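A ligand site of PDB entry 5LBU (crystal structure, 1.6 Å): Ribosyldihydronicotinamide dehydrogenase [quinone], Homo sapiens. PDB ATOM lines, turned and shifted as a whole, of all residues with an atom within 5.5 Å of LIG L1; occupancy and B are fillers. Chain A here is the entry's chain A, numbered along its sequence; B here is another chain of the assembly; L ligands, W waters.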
ATOM      1  N   HIS A  12      16.126 -15.027  -6.375  1.00  0.00           N
ATOM      2  CA  HIS A  12      17.049 -16.038  -6.872  1.00  0.00           C
ATOM      3  C   HIS A  12      17.070 -17.233  -5.916  1.00  0.00           C
ATOM      4  O   HIS A  12      17.023 -17.064  -4.715  1.00  0.00           O
ATOM      5  CB  HIS A  12      18.456 -15.521  -7.134  1.00  0.00           C
ATOM      6  CG  HIS A  12      19.204 -16.357  -8.123  1.00  0.00           C
ATOM      7  ND1 HIS A  12      19.721 -17.587  -7.819  1.00  0.00           N
ATOM      8  CD2 HIS A  12      19.517 -16.124  -9.424  1.00  0.00           C
ATOM      9  CE1 HIS A  12      20.329 -18.087  -8.884  1.00  0.00           C
ATOM     10  NE2 HIS A  12      20.217 -17.215  -9.864  1.00  0.00           N
ATOM     11  N   LYS A  16      24.691 -18.564  -3.525  1.00  0.00           N
ATOM     12  CA  LYS A  16      26.022 -18.461  -4.137  1.00  0.00           C
ATOM     13  C   LYS A  16      26.017 -17.943  -5.581  1.00  0.00           C
ATOM     14  O   LYS A  16      27.061 -17.820  -6.204  1.00  0.00           O
ATOM     15  CB  LYS A  16      26.719 -19.819  -4.075  1.00  0.00           C
ATOM     16  CG  LYS A  16      26.971 -20.285  -2.642  1.00  0.00           C
ATOM     17  CD  LYS A  16      27.469 -21.725  -2.589  1.00  0.00           C
ATOM     18  CE  LYS A  16      28.013 -22.033  -1.194  1.00  0.00           C
ATOM     19  NZ  LYS A  16      28.526 -23.427  -1.082  1.00  0.00           N
ATOM     20  N   SER A  17      24.834 -17.642  -6.105  1.00  0.00           N
ATOM     21  CA  SER A  17      24.696 -17.144  -7.463  1.00  0.00           C
ATOM     22  C   SER A  17      25.240 -15.734  -7.588  1.00  0.00           C
ATOM     23  O   SER A  17      25.480 -15.052  -6.604  1.00  0.00           O
ATOM     24  CB  SER A  17      23.229 -17.152  -7.882  1.00  0.00           C
ATOM     25  OG  SER A  17      22.442 -16.232  -7.126  1.00  0.00           O
ATOM     26  N   PHE A  18      25.394 -15.291  -8.835  1.00  0.00           N
ATOM     27  CA  PHE A  18      25.778 -13.922  -9.111  1.00  0.00           C
ATOM     28  C   PHE A  18      24.727 -12.956  -8.543  1.00  0.00           C
ATOM     29  O   PHE A  18      25.087 -11.939  -7.925  1.00  0.00           O
ATOM     30  CB  PHE A  18      25.998 -13.689 -10.607  1.00  0.00           C
ATOM     31  CG  PHE A  18      26.735 -12.431 -10.906  1.00  0.00           C
ATOM     32  CD1 PHE A  18      28.092 -12.345 -10.665  1.00  0.00           C
ATOM     33  CD2 PHE A  18      26.073 -11.311 -11.367  1.00  0.00           C
ATOM     34  CE1 PHE A  18      28.797 -11.182 -10.924  1.00  0.00           C
ATOM     35  CE2 PHE A  18      26.770 -10.136 -11.627  1.00  0.00           C
ATOM     36  CZ  PHE A  18      28.132 -10.068 -11.408  1.00  0.00           C
ATOM     37  N   ASN A  19      23.450 -13.288  -8.708  1.00  0.00           N
ATOM     38  CA  ASN A  19      22.374 -12.506  -8.084  1.00  0.00           C
ATOM     39  C   ASN A  19      22.525 -12.464  -6.572  1.00  0.00           C
ATOM     40  O   ASN A  19      22.402 -11.393  -5.989  1.00  0.00           O
ATOM     41  CB  ASN A  19      20.993 -13.043  -8.414  1.00  0.00           C
ATOM     42  CG  ASN A  19      20.438 -12.454  -9.694  1.00  0.00           C
ATOM     43  OD1 ASN A  19      19.661 -11.496  -9.652  1.00  0.00           O
ATOM     44  ND2 ASN A  19      20.868 -12.997 -10.832  1.00  0.00           N
ATOM     45  N   GLY A  20      22.807 -13.612  -5.957  1.00  0.00           N
ATOM     46  CA  GLY A  20      23.072 -13.673  -4.510  1.00  0.00           C
ATOM     47  C   GLY A  20      24.194 -12.760  -4.062  1.00  0.00           C
ATOM     48  O   GLY A  20      24.083 -12.077  -3.033  1.00  0.00           O
ATOM     49  N   SER A  21      25.282 -12.745  -4.854  1.00  0.00           N
ATOM     50  CA  SER A  21      26.410 -11.853  -4.625  1.00  0.00           C
ATOM     51  C   SER A  21      26.040 -10.384  -4.735  1.00  0.00           C
ATOM     52  O   SER A  21      26.494  -9.576  -3.929  1.00  0.00           O
ATOM     53  CB  SER A  21      27.577 -12.172  -5.566  1.00  0.00           C
ATOM     54  OG  SER A  21      28.138 -13.430  -5.248  1.00  0.00           O
ATOM     55  N   PRO A 103      17.354 -12.270 -11.897  1.00  0.00           N
ATOM     56  CA  PRO A 103      17.724 -12.642 -13.239  1.00  0.00           C
ATOM     57  C   PRO A 103      16.567 -12.427 -14.210  1.00  0.00           C
ATOM     58  O   PRO A 103      15.383 -12.666 -13.868  1.00  0.00           O
ATOM     59  CB  PRO A 103      18.064 -14.129 -13.103  1.00  0.00           C
ATOM     60  CG  PRO A 103      17.090 -14.603 -12.069  1.00  0.00           C
ATOM     61  CD  PRO A 103      17.002 -13.465 -11.092  1.00  0.00           C
ATOM     62  N   LEU A 104      16.892 -11.977 -15.414  1.00  0.00           N
ATOM     63  CA  LEU A 104      15.892 -11.783 -16.459  1.00  0.00           C
ATOM     64  C   LEU A 104      15.331 -13.141 -16.884  1.00  0.00           C
ATOM     65  O   LEU A 104      16.088 -14.043 -17.259  1.00  0.00           O
ATOM     66  CB  LEU A 104      16.528 -11.061 -17.668  1.00  0.00           C
ATOM     67  CG  LEU A 104      15.580 -10.519 -18.738  1.00  0.00           C
ATOM     68  CD1 LEU A 104      14.768  -9.348 -18.231  1.00  0.00           C
ATOM     69  CD2 LEU A 104      16.391 -10.084 -19.954  1.00  0.00           C
ATOM     70  N   TYR A 105      14.007 -13.289 -16.766  1.00  0.00           N
ATOM     71  CA  TYR A 105      13.290 -14.467 -17.239  1.00  0.00           C
ATOM     72  C   TYR A 105      12.314 -14.005 -18.299  1.00  0.00           C
ATOM     73  O   TYR A 105      11.368 -13.274 -17.980  1.00  0.00           O
ATOM     74  CB  TYR A 105      12.507 -15.168 -16.119  1.00  0.00           C
ATOM     75  CG  TYR A 105      13.261 -16.124 -15.189  1.00  0.00           C
ATOM     76  CD1 TYR A 105      14.651 -16.151 -15.090  1.00  0.00           C
ATOM     77  CD2 TYR A 105      12.540 -16.992 -14.361  1.00  0.00           C
ATOM     78  CE1 TYR A 105      15.293 -17.009 -14.199  1.00  0.00           C
ATOM     79  CE2 TYR A 105      13.176 -17.848 -13.483  1.00  0.00           C
ATOM     80  CZ  TYR A 105      14.552 -17.860 -13.399  1.00  0.00           C
ATOM     81  OH  TYR A 105      15.155 -18.724 -12.531  1.00  0.00           O
ATOM     82  N   TRP A 106      12.516 -14.453 -19.528  1.00  0.00           N
ATOM     83  CA  TRP A 106      11.606 -14.143 -20.636  1.00  0.00           C
ATOM     84  C   TRP A 106      11.334 -12.632 -20.756  1.00  0.00           C
ATOM     85  O   TRP A 106      10.176 -12.177 -20.744  1.00  0.00           O
ATOM     86  CB  TRP A 106      10.315 -14.964 -20.500  1.00  0.00           C
ATOM     87  CG  TRP A 106      10.547 -16.418 -20.728  1.00  0.00           C
ATOM     88  CD1 TRP A 106      10.310 -17.441 -19.848  1.00  0.00           C
ATOM     89  CD2 TRP A 106      11.109 -17.011 -21.896  1.00  0.00           C
ATOM     90  NE1 TRP A 106      10.680 -18.638 -20.411  1.00  0.00           N
ATOM     91  CE2 TRP A 106      11.174 -18.401 -21.673  1.00  0.00           C
ATOM     92  CE3 TRP A 106      11.555 -16.506 -23.124  1.00  0.00           C
ATOM     93  CZ2 TRP A 106      11.663 -19.285 -22.628  1.00  0.00           C
ATOM     94  CZ3 TRP A 106      12.049 -17.385 -24.073  1.00  0.00           C
ATOM     95  CH2 TRP A 106      12.106 -18.756 -23.811  1.00  0.00           C
ATOM     96  N   PHE A 107      12.428 -11.863 -20.831  1.00  0.00           N
ATOM     97  CA  PHE A 107      12.375 -10.411 -20.991  1.00  0.00           C
ATOM     98  C   PHE A 107      11.613  -9.727 -19.841  1.00  0.00           C
ATOM     99  O   PHE A 107      11.008  -8.663 -20.016  1.00  0.00           O
ATOM    100  CB  PHE A 107      11.695 -10.027 -22.341  1.00  0.00           C
ATOM    101  CG  PHE A 107      12.621 -10.016 -23.543  1.00  0.00           C
ATOM    102  CD1 PHE A 107      13.628 -10.942 -23.704  1.00  0.00           C
ATOM    103  CD2 PHE A 107      12.396  -9.092 -24.572  1.00  0.00           C
ATOM    104  CE1 PHE A 107      14.438 -10.934 -24.848  1.00  0.00           C
ATOM    105  CE2 PHE A 107      13.187  -9.061 -25.703  1.00  0.00           C
ATOM    106  CZ  PHE A 107      14.219  -9.983 -25.842  1.00  0.00           C
ATOM    107  N   SER A 108      11.597 -10.354 -18.664  1.00  0.00           N
ATOM    108  CA  SER A 108      10.770  -9.864 -17.567  1.00  0.00           C
ATOM    109  C   SER A 108      11.320 -10.398 -16.249  1.00  0.00           C
ATOM    110  O   SER A 108      12.450 -10.896 -16.187  1.00  0.00           O
ATOM    111  CB  SER A 108       9.319 -10.280 -17.808  1.00  0.00           C
ATOM    112  OG  SER A 108       8.447  -9.784 -16.800  1.00  0.00           O
ATOM    113  N   THR A 148      20.160  -9.248 -14.018  1.00  0.00           N
ATOM    114  CA  THR A 148      21.238  -9.984 -14.697  1.00  0.00           C
ATOM    115  C   THR A 148      20.653 -10.645 -15.933  1.00  0.00           C
ATOM    116  O   THR A 148      19.468 -10.999 -15.931  1.00  0.00           O
ATOM    117  CB  THR A 148      21.863 -11.052 -13.782  1.00  0.00           C
ATOM    118  OG1 THR A 148      20.878 -12.031 -13.423  1.00  0.00           O
ATOM    119  CG2 THR A 148      22.454 -10.434 -12.502  1.00  0.00           C
ATOM    120  N   THR A 149      21.455 -10.845 -16.970  1.00  0.00           N
ATOM    121  CA  THR A 149      20.950 -11.433 -18.227  1.00  0.00           C
ATOM    122  C   THR A 149      21.790 -12.610 -18.677  1.00  0.00           C
ATOM    123  O   THR A 149      22.939 -12.777 -18.259  1.00  0.00           O
ATOM    124  CB  THR A 149      20.948 -10.412 -19.371  1.00  0.00           C
ATOM    125  OG1 THR A 149      22.297 -10.039 -19.671  1.00  0.00           O
ATOM    126  CG2 THR A 149      20.144  -9.164 -19.024  1.00  0.00           C
ATOM    127  N   GLY A 150      21.210 -13.430 -19.549  1.00  0.00           N
ATOM    128  CA  GLY A 150      21.968 -14.423 -20.300  1.00  0.00           C
ATOM    129  C   GLY A 150      22.711 -13.773 -21.454  1.00  0.00           C
ATOM    130  O   GLY A 150      23.857 -14.108 -21.719  1.00  0.00           O
ATOM    131  N   GLY A 151      22.050 -12.834 -22.129  1.00  0.00           N
ATOM    132  CA  GLY A 151      22.624 -12.140 -23.294  1.00  0.00           C
ATOM    133  C   GLY A 151      23.654 -11.066 -22.966  1.00  0.00           C
ATOM    134  O   GLY A 151      23.600 -10.418 -21.915  1.00  0.00           O
ATOM    135  N   TYR A 156      21.924  -6.758 -26.878  1.00  0.00           N
ATOM    136  CA  TYR A 156      20.806  -5.929 -26.438  1.00  0.00           C
ATOM    137  C   TYR A 156      20.931  -4.500 -26.996  1.00  0.00           C
ATOM    138  O   TYR A 156      20.825  -3.518 -26.266  1.00  0.00           O
ATOM    139  CB  TYR A 156      20.669  -6.000 -24.894  1.00  0.00           C
ATOM    140  CG  TYR A 156      19.978  -7.275 -24.407  1.00  0.00           C
ATOM    141  CD1 TYR A 156      18.632  -7.481 -24.687  1.00  0.00           C
ATOM    142  CD2 TYR A 156      20.657  -8.271 -23.674  1.00  0.00           C
ATOM    143  CE1 TYR A 156      17.965  -8.619 -24.266  1.00  0.00           C
ATOM    144  CE2 TYR A 156      19.987  -9.430 -23.264  1.00  0.00           C
ATOM    145  CZ  TYR A 156      18.647  -9.599 -23.562  1.00  0.00           C
ATOM    146  OH  TYR A 156      17.913 -10.722 -23.188  1.00  0.00           O
ATOM    147  N   PRO A 193      26.704 -12.680 -16.870  1.00  0.00           N
ATOM    148  CA  PRO A 193      27.721 -13.157 -15.926  1.00  0.00           C
ATOM    149  C   PRO A 193      28.161 -14.618 -16.144  1.00  0.00           C
ATOM    150  O   PRO A 193      29.304 -14.949 -15.854  1.00  0.00           O
ATOM    151  CB  PRO A 193      27.071 -12.955 -14.561  1.00  0.00           C
ATOM    152  CG  PRO A 193      25.612 -12.847 -14.832  1.00  0.00           C
ATOM    153  CD  PRO A 193      25.516 -12.183 -16.157  1.00  0.00           C
ATOM    154  N   GLU A 194      27.273 -15.471 -16.659  1.00  0.00           N
ATOM    155  CA  GLU A 194      27.625 -16.869 -16.912  1.00  0.00           C
ATOM    156  C   GLU A 194      28.672 -16.992 -18.008  1.00  0.00           C
ATOM    157  O   GLU A 194      29.512 -17.872 -17.951  1.00  0.00           O
ATOM    158  CB  GLU A 194      26.402 -17.693 -17.280  1.00  0.00           C
ATOM    159  CG  GLU A 194      25.359 -17.828 -16.172  1.00  0.00           C
ATOM    160  CD  GLU A 194      24.014 -18.291 -16.698  1.00  0.00           C
ATOM    161  OE1 GLU A 194      23.331 -17.490 -17.371  1.00  0.00           O
ATOM    162  OE2 GLU A 194      23.647 -19.451 -16.446  1.00  0.00           O
ATOM    163  N   GLU A 198      35.771 -14.434 -14.997  1.00  0.00           N
ATOM    164  CA  GLU A 198      35.874 -14.182 -13.560  1.00  0.00           C
ATOM    165  C   GLU A 198      36.145 -12.708 -13.249  1.00  0.00           C
ATOM    166  O   GLU A 198      35.473 -12.103 -12.409  1.00  0.00           O
ATOM    167  CB  GLU A 198      36.996 -15.069 -12.973  1.00  0.00           C
ATOM    168  CG  GLU A 198      37.295 -14.907 -11.484  1.00  0.00           C
ATOM    169  CD  GLU A 198      36.123 -15.235 -10.575  1.00  0.00           C
ATOM    170  OE1 GLU A 198      35.206 -15.977 -10.982  1.00  0.00           O
ATOM    171  OE2 GLU A 198      36.130 -14.763  -9.425  1.00  0.00           O
ATOM    172  N   ARG A 201      33.263 -10.449 -14.056  1.00  0.00           N
ATOM    173  CA  ARG A 201      32.237 -10.574 -13.016  1.00  0.00           C
ATOM    174  C   ARG A 201      32.598  -9.743 -11.792  1.00  0.00           C
ATOM    175  O   ARG A 201      31.742  -9.074 -11.211  1.00  0.00           O
ATOM    176  CB  ARG A 201      32.021 -12.044 -12.640  1.00  0.00           C
ATOM    177  CG  ARG A 201      31.224 -12.817 -13.682  1.00  0.00           C
ATOM    178  CD  ARG A 201      30.844 -14.223 -13.211  1.00  0.00           C
ATOM    179  NE  ARG A 201      31.646 -15.286 -13.824  1.00  0.00           N
ATOM    180  CZ  ARG A 201      32.618 -15.990 -13.234  1.00  0.00           C
ATOM    181  NH1 ARG A 201      32.960 -15.787 -11.968  1.00  0.00           N
ATOM    182  NH2 ARG A 201      33.252 -16.930 -13.919  1.00  0.00           N
ATOM    183  N   LYS A 202      33.868  -9.801 -11.395  1.00  0.00           N
ATOM    184  CA  LYS A 202      34.372  -9.000 -10.289  1.00  0.00           C
ATOM    185  C   LYS A 202      34.178  -7.505 -10.542  1.00  0.00           C
ATOM    186  O   LYS A 202      33.747  -6.755  -9.642  1.00  0.00           O
ATOM    187  CB  LYS A 202      35.853  -9.303 -10.024  1.00  0.00           C
ATOM    188  CG  LYS A 202      36.136 -10.684  -9.446  1.00  0.00           C
ATOM    189  CD  LYS A 202      35.562 -10.834  -8.042  1.00  0.00           C
ATOM    190  CE  LYS A 202      35.978 -12.121  -7.360  1.00  0.00           C
ATOM    191  NZ  LYS A 202      35.043 -12.467  -6.244  1.00  0.00           N
ATOM    192  N   VAL A 205      30.520  -6.653 -10.009  1.00  0.00           N
ATOM    193  CA  VAL A 205      30.210  -6.565  -8.576  1.00  0.00           C
ATOM    194  C   VAL A 205      30.747  -5.247  -8.007  1.00  0.00           C
ATOM    195  O   VAL A 205      30.023  -4.531  -7.285  1.00  0.00           O
ATOM    196  CB  VAL A 205      30.779  -7.761  -7.775  1.00  0.00           C
ATOM    197  CG1 VAL A 205      30.496  -7.586  -6.294  1.00  0.00           C
ATOM    198  CG2 VAL A 205      30.158  -9.059  -8.269  1.00  0.00           C
ATOM    199  N   ASN B  67      21.626 -23.886 -10.482  1.00  0.00           N
ATOM    200  CA  ASN B  67      21.360 -22.988 -11.609  1.00  0.00           C
ATOM    201  C   ASN B  67      20.142 -23.541 -12.345  1.00  0.00           C
ATOM    202  O   ASN B  67      20.245 -24.562 -13.027  1.00  0.00           O
ATOM    203  CB  ASN B  67      22.588 -22.971 -12.525  1.00  0.00           C
ATOM    204  CG  ASN B  67      22.431 -22.051 -13.719  1.00  0.00           C
ATOM    205  OD1 ASN B  67      21.366 -21.970 -14.342  1.00  0.00           O
ATOM    206  ND2 ASN B  67      23.516 -21.357 -14.067  1.00  0.00           N
ATOM    207  N   TYR B  68      18.995 -22.870 -12.218  1.00  0.00           N
ATOM    208  CA  TYR B  68      17.718 -23.363 -12.750  1.00  0.00           C
ATOM    209  C   TYR B  68      17.763 -23.656 -14.239  1.00  0.00           C
ATOM    210  O   TYR B  68      17.285 -24.695 -14.676  1.00  0.00           O
ATOM    211  CB  TYR B  68      16.554 -22.410 -12.428  1.00  0.00           C
ATOM    212  CG  TYR B  68      15.197 -22.972 -12.805  1.00  0.00           C
ATOM    213  CD1 TYR B  68      14.520 -23.838 -11.942  1.00  0.00           C
ATOM    214  CD2 TYR B  68      14.593 -22.673 -14.034  1.00  0.00           C
ATOM    215  CE1 TYR B  68      13.277 -24.375 -12.285  1.00  0.00           C
ATOM    216  CE2 TYR B  68      13.364 -23.200 -14.382  1.00  0.00           C
ATOM    217  CZ  TYR B  68      12.697 -24.047 -13.494  1.00  0.00           C
ATOM    218  OH  TYR B  68      11.495 -24.593 -13.866  1.00  0.00           O
ATOM    219  N   GLY B  69      18.322 -22.732 -15.030  1.00  0.00           N
ATOM    220  CA  GLY B  69      18.430 -22.922 -16.484  1.00  0.00           C
ATOM    221  C   GLY B  69      19.259 -24.150 -16.869  1.00  0.00           C
ATOM    222  O   GLY B  69      18.817 -25.010 -17.677  1.00  0.00           O
ATOM    223  N   ASP B 118       7.917 -19.664 -17.693  1.00  0.00           N
ATOM    224  CA  ASP B 118       9.221 -19.928 -17.088  1.00  0.00           C
ATOM    225  C   ASP B 118       9.571 -21.418 -17.021  1.00  0.00           C
ATOM    226  O   ASP B 118      10.697 -21.805 -17.304  1.00  0.00           O
ATOM    227  CB  ASP B 118       9.299 -19.363 -15.657  1.00  0.00           C
ATOM    228  CG  ASP B 118       9.227 -17.838 -15.595  1.00  0.00           C
ATOM    229  OD1 ASP B 118       9.359 -17.150 -16.628  1.00  0.00           O
ATOM    230  OD2 ASP B 118       9.047 -17.305 -14.482  1.00  0.00           O
ATOM    231  N   GLY B 175      10.075 -11.576 -27.229  1.00  0.00           N
ATOM    232  CA  GLY B 175      11.036 -12.083 -26.275  1.00  0.00           C
ATOM    233  C   GLY B 175      10.766 -13.508 -25.810  1.00  0.00           C
ATOM    234  O   GLY B 175      11.700 -14.213 -25.448  1.00  0.00           O
HETATM  235  P1  LIG L   1      25.115 -17.490 -11.991  1.00  0.00           P
HETATM  236  O1  LIG L   1      25.125 -18.673 -12.896  1.00  0.00           O
HETATM  237  O2  LIG L   1      24.796 -17.654 -10.554  1.00  0.00           O
HETATM  238  O3  LIG L   1      26.530 -16.764 -12.068  1.00  0.00           O
HETATM  239  C1  LIG L   1      27.468 -16.971 -13.095  1.00  0.00           C
HETATM  240  C2  LIG L   1      28.832 -17.132 -12.440  1.00  0.00           C
HETATM  241  O4  LIG L   1      29.103 -16.051 -11.562  1.00  0.00           O
HETATM  242  C3  LIG L   1      28.876 -18.388 -11.594  1.00  0.00           C
HETATM  243  O5  LIG L   1      30.015 -19.103 -12.018  1.00  0.00           O
HETATM  244  C4  LIG L   1      29.061 -17.871 -10.173  1.00  0.00           C
HETATM  245  O6  LIG L   1      29.846 -18.737  -9.371  1.00  0.00           O
HETATM  246  C5  LIG L   1      29.783 -16.575 -10.441  1.00  0.00           C
HETATM  247  N1  LIG L   1      29.815 -15.642  -9.301  1.00  0.00           N
HETATM  248  C6  LIG L   1      28.955 -15.555  -8.280  1.00  0.00           C
HETATM  249  N2  LIG L   1      29.313 -14.590  -7.419  1.00  0.00           N
HETATM  250  C7  LIG L   1      30.439 -14.043  -7.890  1.00  0.00           C
HETATM  251  C8  LIG L   1      31.361 -12.970  -7.467  1.00  0.00           C
HETATM  252  N3  LIG L   1      31.140 -12.264  -6.346  1.00  0.00           N
HETATM  253  N4  LIG L   1      32.422 -12.727  -8.244  1.00  0.00           N
HETATM  254  C9  LIG L   1      32.655 -13.407  -9.365  1.00  0.00           C
HETATM  255  N5  LIG L   1      31.870 -14.386  -9.812  1.00  0.00           N
HETATM  256  C10 LIG L   1      30.771 -14.749  -9.123  1.00  0.00           C
HETATM  257  N6  LIG L   1      18.382 -14.347 -20.366  1.00  0.00           N
HETATM  258  C11 LIG L   1      18.098 -13.354 -21.242  1.00  0.00           C
HETATM  259  O7  LIG L   1      19.022 -12.641 -21.634  1.00  0.00           O
HETATM  260  N7  LIG L   1      16.864 -13.102 -21.683  1.00  0.00           N
HETATM  261  C12 LIG L   1      15.815 -13.828 -21.310  1.00  0.00           C
HETATM  262  O8  LIG L   1      14.673 -13.595 -21.725  1.00  0.00           O
HETATM  263  C13 LIG L   1      16.042 -14.929 -20.361  1.00  0.00           C
HETATM  264  N8  LIG L   1      15.048 -15.704 -19.937  1.00  0.00           N
HETATM  265  C14 LIG L   1      15.282 -16.698 -19.062  1.00  0.00           C
HETATM  266  C15 LIG L   1      14.237 -17.489 -18.627  1.00  0.00           C
HETATM  267  C16 LIG L   1      14.443 -18.517 -17.731  1.00  0.00           C
HETATM  268  C17 LIG L   1      13.293 -19.363 -17.269  1.00  0.00           C
HETATM  269  C18 LIG L   1      15.802 -18.795 -17.240  1.00  0.00           C
HETATM  270  C19 LIG L   1      16.012 -19.920 -16.258  1.00  0.00           C
HETATM  271  C20 LIG L   1      16.854 -18.015 -17.674  1.00  0.00           C
HETATM  272  C21 LIG L   1      16.646 -16.978 -18.559  1.00  0.00           C
HETATM  273  N9  LIG L   1      17.707 -16.178 -19.015  1.00  0.00           N
HETATM  274  C22 LIG L   1      17.426 -15.140 -19.899  1.00  0.00           C
HETATM  275  C23 LIG L   1      19.060 -16.399 -18.533  1.00  0.00           C
HETATM  276  C24 LIG L   1      19.201 -15.737 -17.155  1.00  0.00           C
HETATM  277  O9  LIG L   1      18.793 -14.376 -17.225  1.00  0.00           O
HETATM  278  C25 LIG L   1      20.625 -15.859 -16.644  1.00  0.00           C
HETATM  279  O10 LIG L   1      20.928 -17.236 -16.530  1.00  0.00           O
HETATM  280  C26 LIG L   1      20.804 -15.206 -15.276  1.00  0.00           C
HETATM  281  O11 LIG L   1      20.610 -13.800 -15.368  1.00  0.00           O
HETATM  282  C27 LIG L   1      22.174 -15.514 -14.695  1.00  0.00           C
HETATM  283  O12 LIG L   1      22.339 -14.961 -13.407  1.00  0.00           O
HETATM  284  P2  LIG L   1      22.726 -15.915 -12.189  1.00  0.00           P
HETATM  285  O13 LIG L   1      22.829 -15.093 -10.964  1.00  0.00           O
HETATM  286  O14 LIG L   1      21.860 -17.108 -12.229  1.00  0.00           O
HETATM  287  O15 LIG L   1      24.200 -16.345 -12.650  1.00  0.00           O
HETATM  288  N1  LG2 L   2      21.701 -17.864 -21.687  1.00  0.00           N
HETATM  289  C1  LG2 L   2      20.297 -17.568 -22.074  1.00  0.00           C
HETATM  290  C2  LG2 L   2      20.039 -16.484 -23.045  1.00  0.00           C
HETATM  291  N2  LG2 L   2      20.763 -15.612 -23.755  1.00  0.00           N
HETATM  292  C3  LG2 L   2      19.894 -14.865 -24.483  1.00  0.00           C
HETATM  293  C4  LG2 L   2      20.318 -13.761 -25.420  1.00  0.00           C
HETATM  294  O1  LG2 L   2      19.869 -13.984 -26.777  1.00  0.00           O
HETATM  295  C5  LG2 L   2      20.188 -15.185 -27.523  1.00  0.00           C
HETATM  296  C6  LG2 L   2      21.149 -16.194 -26.933  1.00  0.00           C
HETATM  297  N3  LG2 L   2      18.622 -15.240 -24.265  1.00  0.00           N
HETATM  298  C7  LG2 L   2      18.642 -16.239 -23.400  1.00  0.00           C
HETATM  299  C8  LG2 L   2      17.624 -16.983 -22.840  1.00  0.00           C
HETATM  300  C9  LG2 L   2      16.297 -16.747 -23.172  1.00  0.00           C
HETATM  301  C10 LG2 L   2      15.301 -17.525 -22.589  1.00  0.00           C
HETATM  302  C11 LG2 L   2      15.616 -18.525 -21.672  1.00  0.00           C
HETATM  303  C12 LG2 L   2      16.943 -18.769 -21.334  1.00  0.00           C
HETATM  304  C13 LG2 L   2      17.955 -18.006 -21.919  1.00  0.00           C
HETATM  305  N4  LG2 L   2      19.246 -18.266 -21.568  1.00  0.00           N
HETATM  306  O   HOH W   1      33.319  -9.954  -5.983  1.00  0.00           O
HETATM  307  O   HOH W   2      12.621 -21.204 -19.636  1.00  0.00           O
HETATM  308  O   HOH W   3      19.200 -17.718 -13.139  1.00  0.00           O
HETATM  309  O   HOH W   4      27.206 -20.502 -13.723  1.00  0.00           O
HETATM  310  O   HOH W   5      14.322 -14.317 -24.396  1.00  0.00           O
HETATM  311  O   HOH W   6      23.228 -20.291  -9.674  1.00  0.00           O
HETATM  312  O   HOH W   7      19.197 -20.222 -18.929  1.00  0.00           O
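The side-chain carboxylate of Glu 194 sits at hydrogen-bond distance from an oxygen (O10) of LIG L1 (2.6 Å). O11 of LIG L1 is in hydrogen-bond range of O of Thr 148, 3.1 Å away. An oxygen (O11) of LIG L1 lies within hydrogen-bond range of the side-chain hydroxyl of Thr 148 (2.6 Å). An oxygen (O7) of LIG L1 is in hydrogen-bond range of the side-chain hydroxyl (OH) of Tyr 156, 2.7 Å away. O of Leu 104 lies within hydrogen-bond range of O9 of LIG L1, at 2.7 Å. A nitrogen (N2) of LIG L1 sits at hydrogen-bond distance from the side-chain hydroxyl (OG) of Ser 21. A nitrogen (N5) of LIG L1 lies within hydrogen-bond range of the guanidinium group (NH1) of Arg 201 (2.8 Å). N of Trp 106 sits at hydrogen-bond distance from N8 of LIG L1, at 2.9 Å. N of Asn 19 sits at hydrogen-bond distance from O13 of LIG L1, at 3.0 Å. The side-chain amide nitrogen of Asn 19 lies within hydrogen-bond range of an oxygen (O13) of LIG L1 (2.9 Å). NE2 of His 12 sits at hydrogen-bond distance from O14 of LIG L1 (2.9 Å). The backbone NH of Phe 107 is in hydrogen-bond range of an oxygen (O8) of LIG L1, 3.0 Å away. The backbone NH (N) of Phe 18 sits at hydrogen-bond distance from an oxygen (O2) of LIG L1 (3.0 Å). An oxygen (O7) of LIG L1 is in hydrogen-bond range of the backbone NH (N) of Gly 151. N6 of LIG L1 lies within hydrogen-bond range of N of Gly 150 (3.1 Å). N4 of LIG L1 lies within hydrogen-bond range of NZ of Lys 202, at 3.3 Å. An oxygen (O1) of LIG L1 is in hydrogen-bond range of the side-chain amide nitrogen (ND2) of Asn 67 of chain B (3.3 Å). N of Thr 149 lies within hydrogen-bond range of O11 of LIG L1 (3.5 Å). A nitrogen (N2) of LG2 L2 lies within hydrogen-bond range of the backbone NH of Gly 151 (3.5 Å).
OE2 of Glu 194 lies within hydrogen-bond range of ND2 of Asn 67 of chain B, 3.1 Å away. The backbone carbonyl oxygen (O) of Thr 148 is in hydrogen-bond range of the backbone NH (N) of Leu 104 (2.8 Å). The side-chain hydroxyl of Ser 21 sits at hydrogen-bond distance from the backbone carbonyl oxygen of Ser 17, 3.4 Å away. NH1 of Arg 201 is in salt-bridge range of OE1 of Glu 198 (2.5 Å). The guanidinium group (NE) of Arg 201 is in hydrogen-bond range of the backbone carbonyl oxygen (O) of Pro 193, at 3.1 Å. The backbone carbonyl oxygen of Gly 151 lies within hydrogen-bond range of the side-chain hydroxyl of Thr 149, 2.6 Å away. N of Gly 20 lies within hydrogen-bond range of OG of Ser 17. N of Gly 69 of chain B lies within hydrogen-bond range of OD1 of Asn 67 of chain B (3.2 Å).
Merely in contact with LIG L1: Lys 16 (3.6 Å), Ser 17 (3.1 Å), Pro 103 (3.4 Å), Tyr 105 (3.4 Å), Pro 193 (3.9 Å), Glu 198 (3.7 Å), Val 205 (3.9 Å), Tyr 68 of chain B (3.8 Å), Gly 69 of chain B (3.8 Å) and Asp 118 of chain B (3.6 Å). Of the 29 residues printed, 26 come within 4 Å of LIG L1. The nearest printed residue that does not touch LIG L1 is Gly 175 of chain B (4.8 Å).
Water W5 bridges O8 of LIG L1 (2.8 Å) and O of Gly 175 of chain B (2.8 Å). Water W3 bridges O14 of LIG L1 (2.9 Å) and NE2 of His 12 (3.5 Å). Water W2 lies within hydrogen-bond range of O of Asp 118 of chain B (3.1 Å) and NE1 of Trp 106 (3.3 Å). Water W1 lies within hydrogen-bond range of NZ of Lys 202 and N3 of LIG L1.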
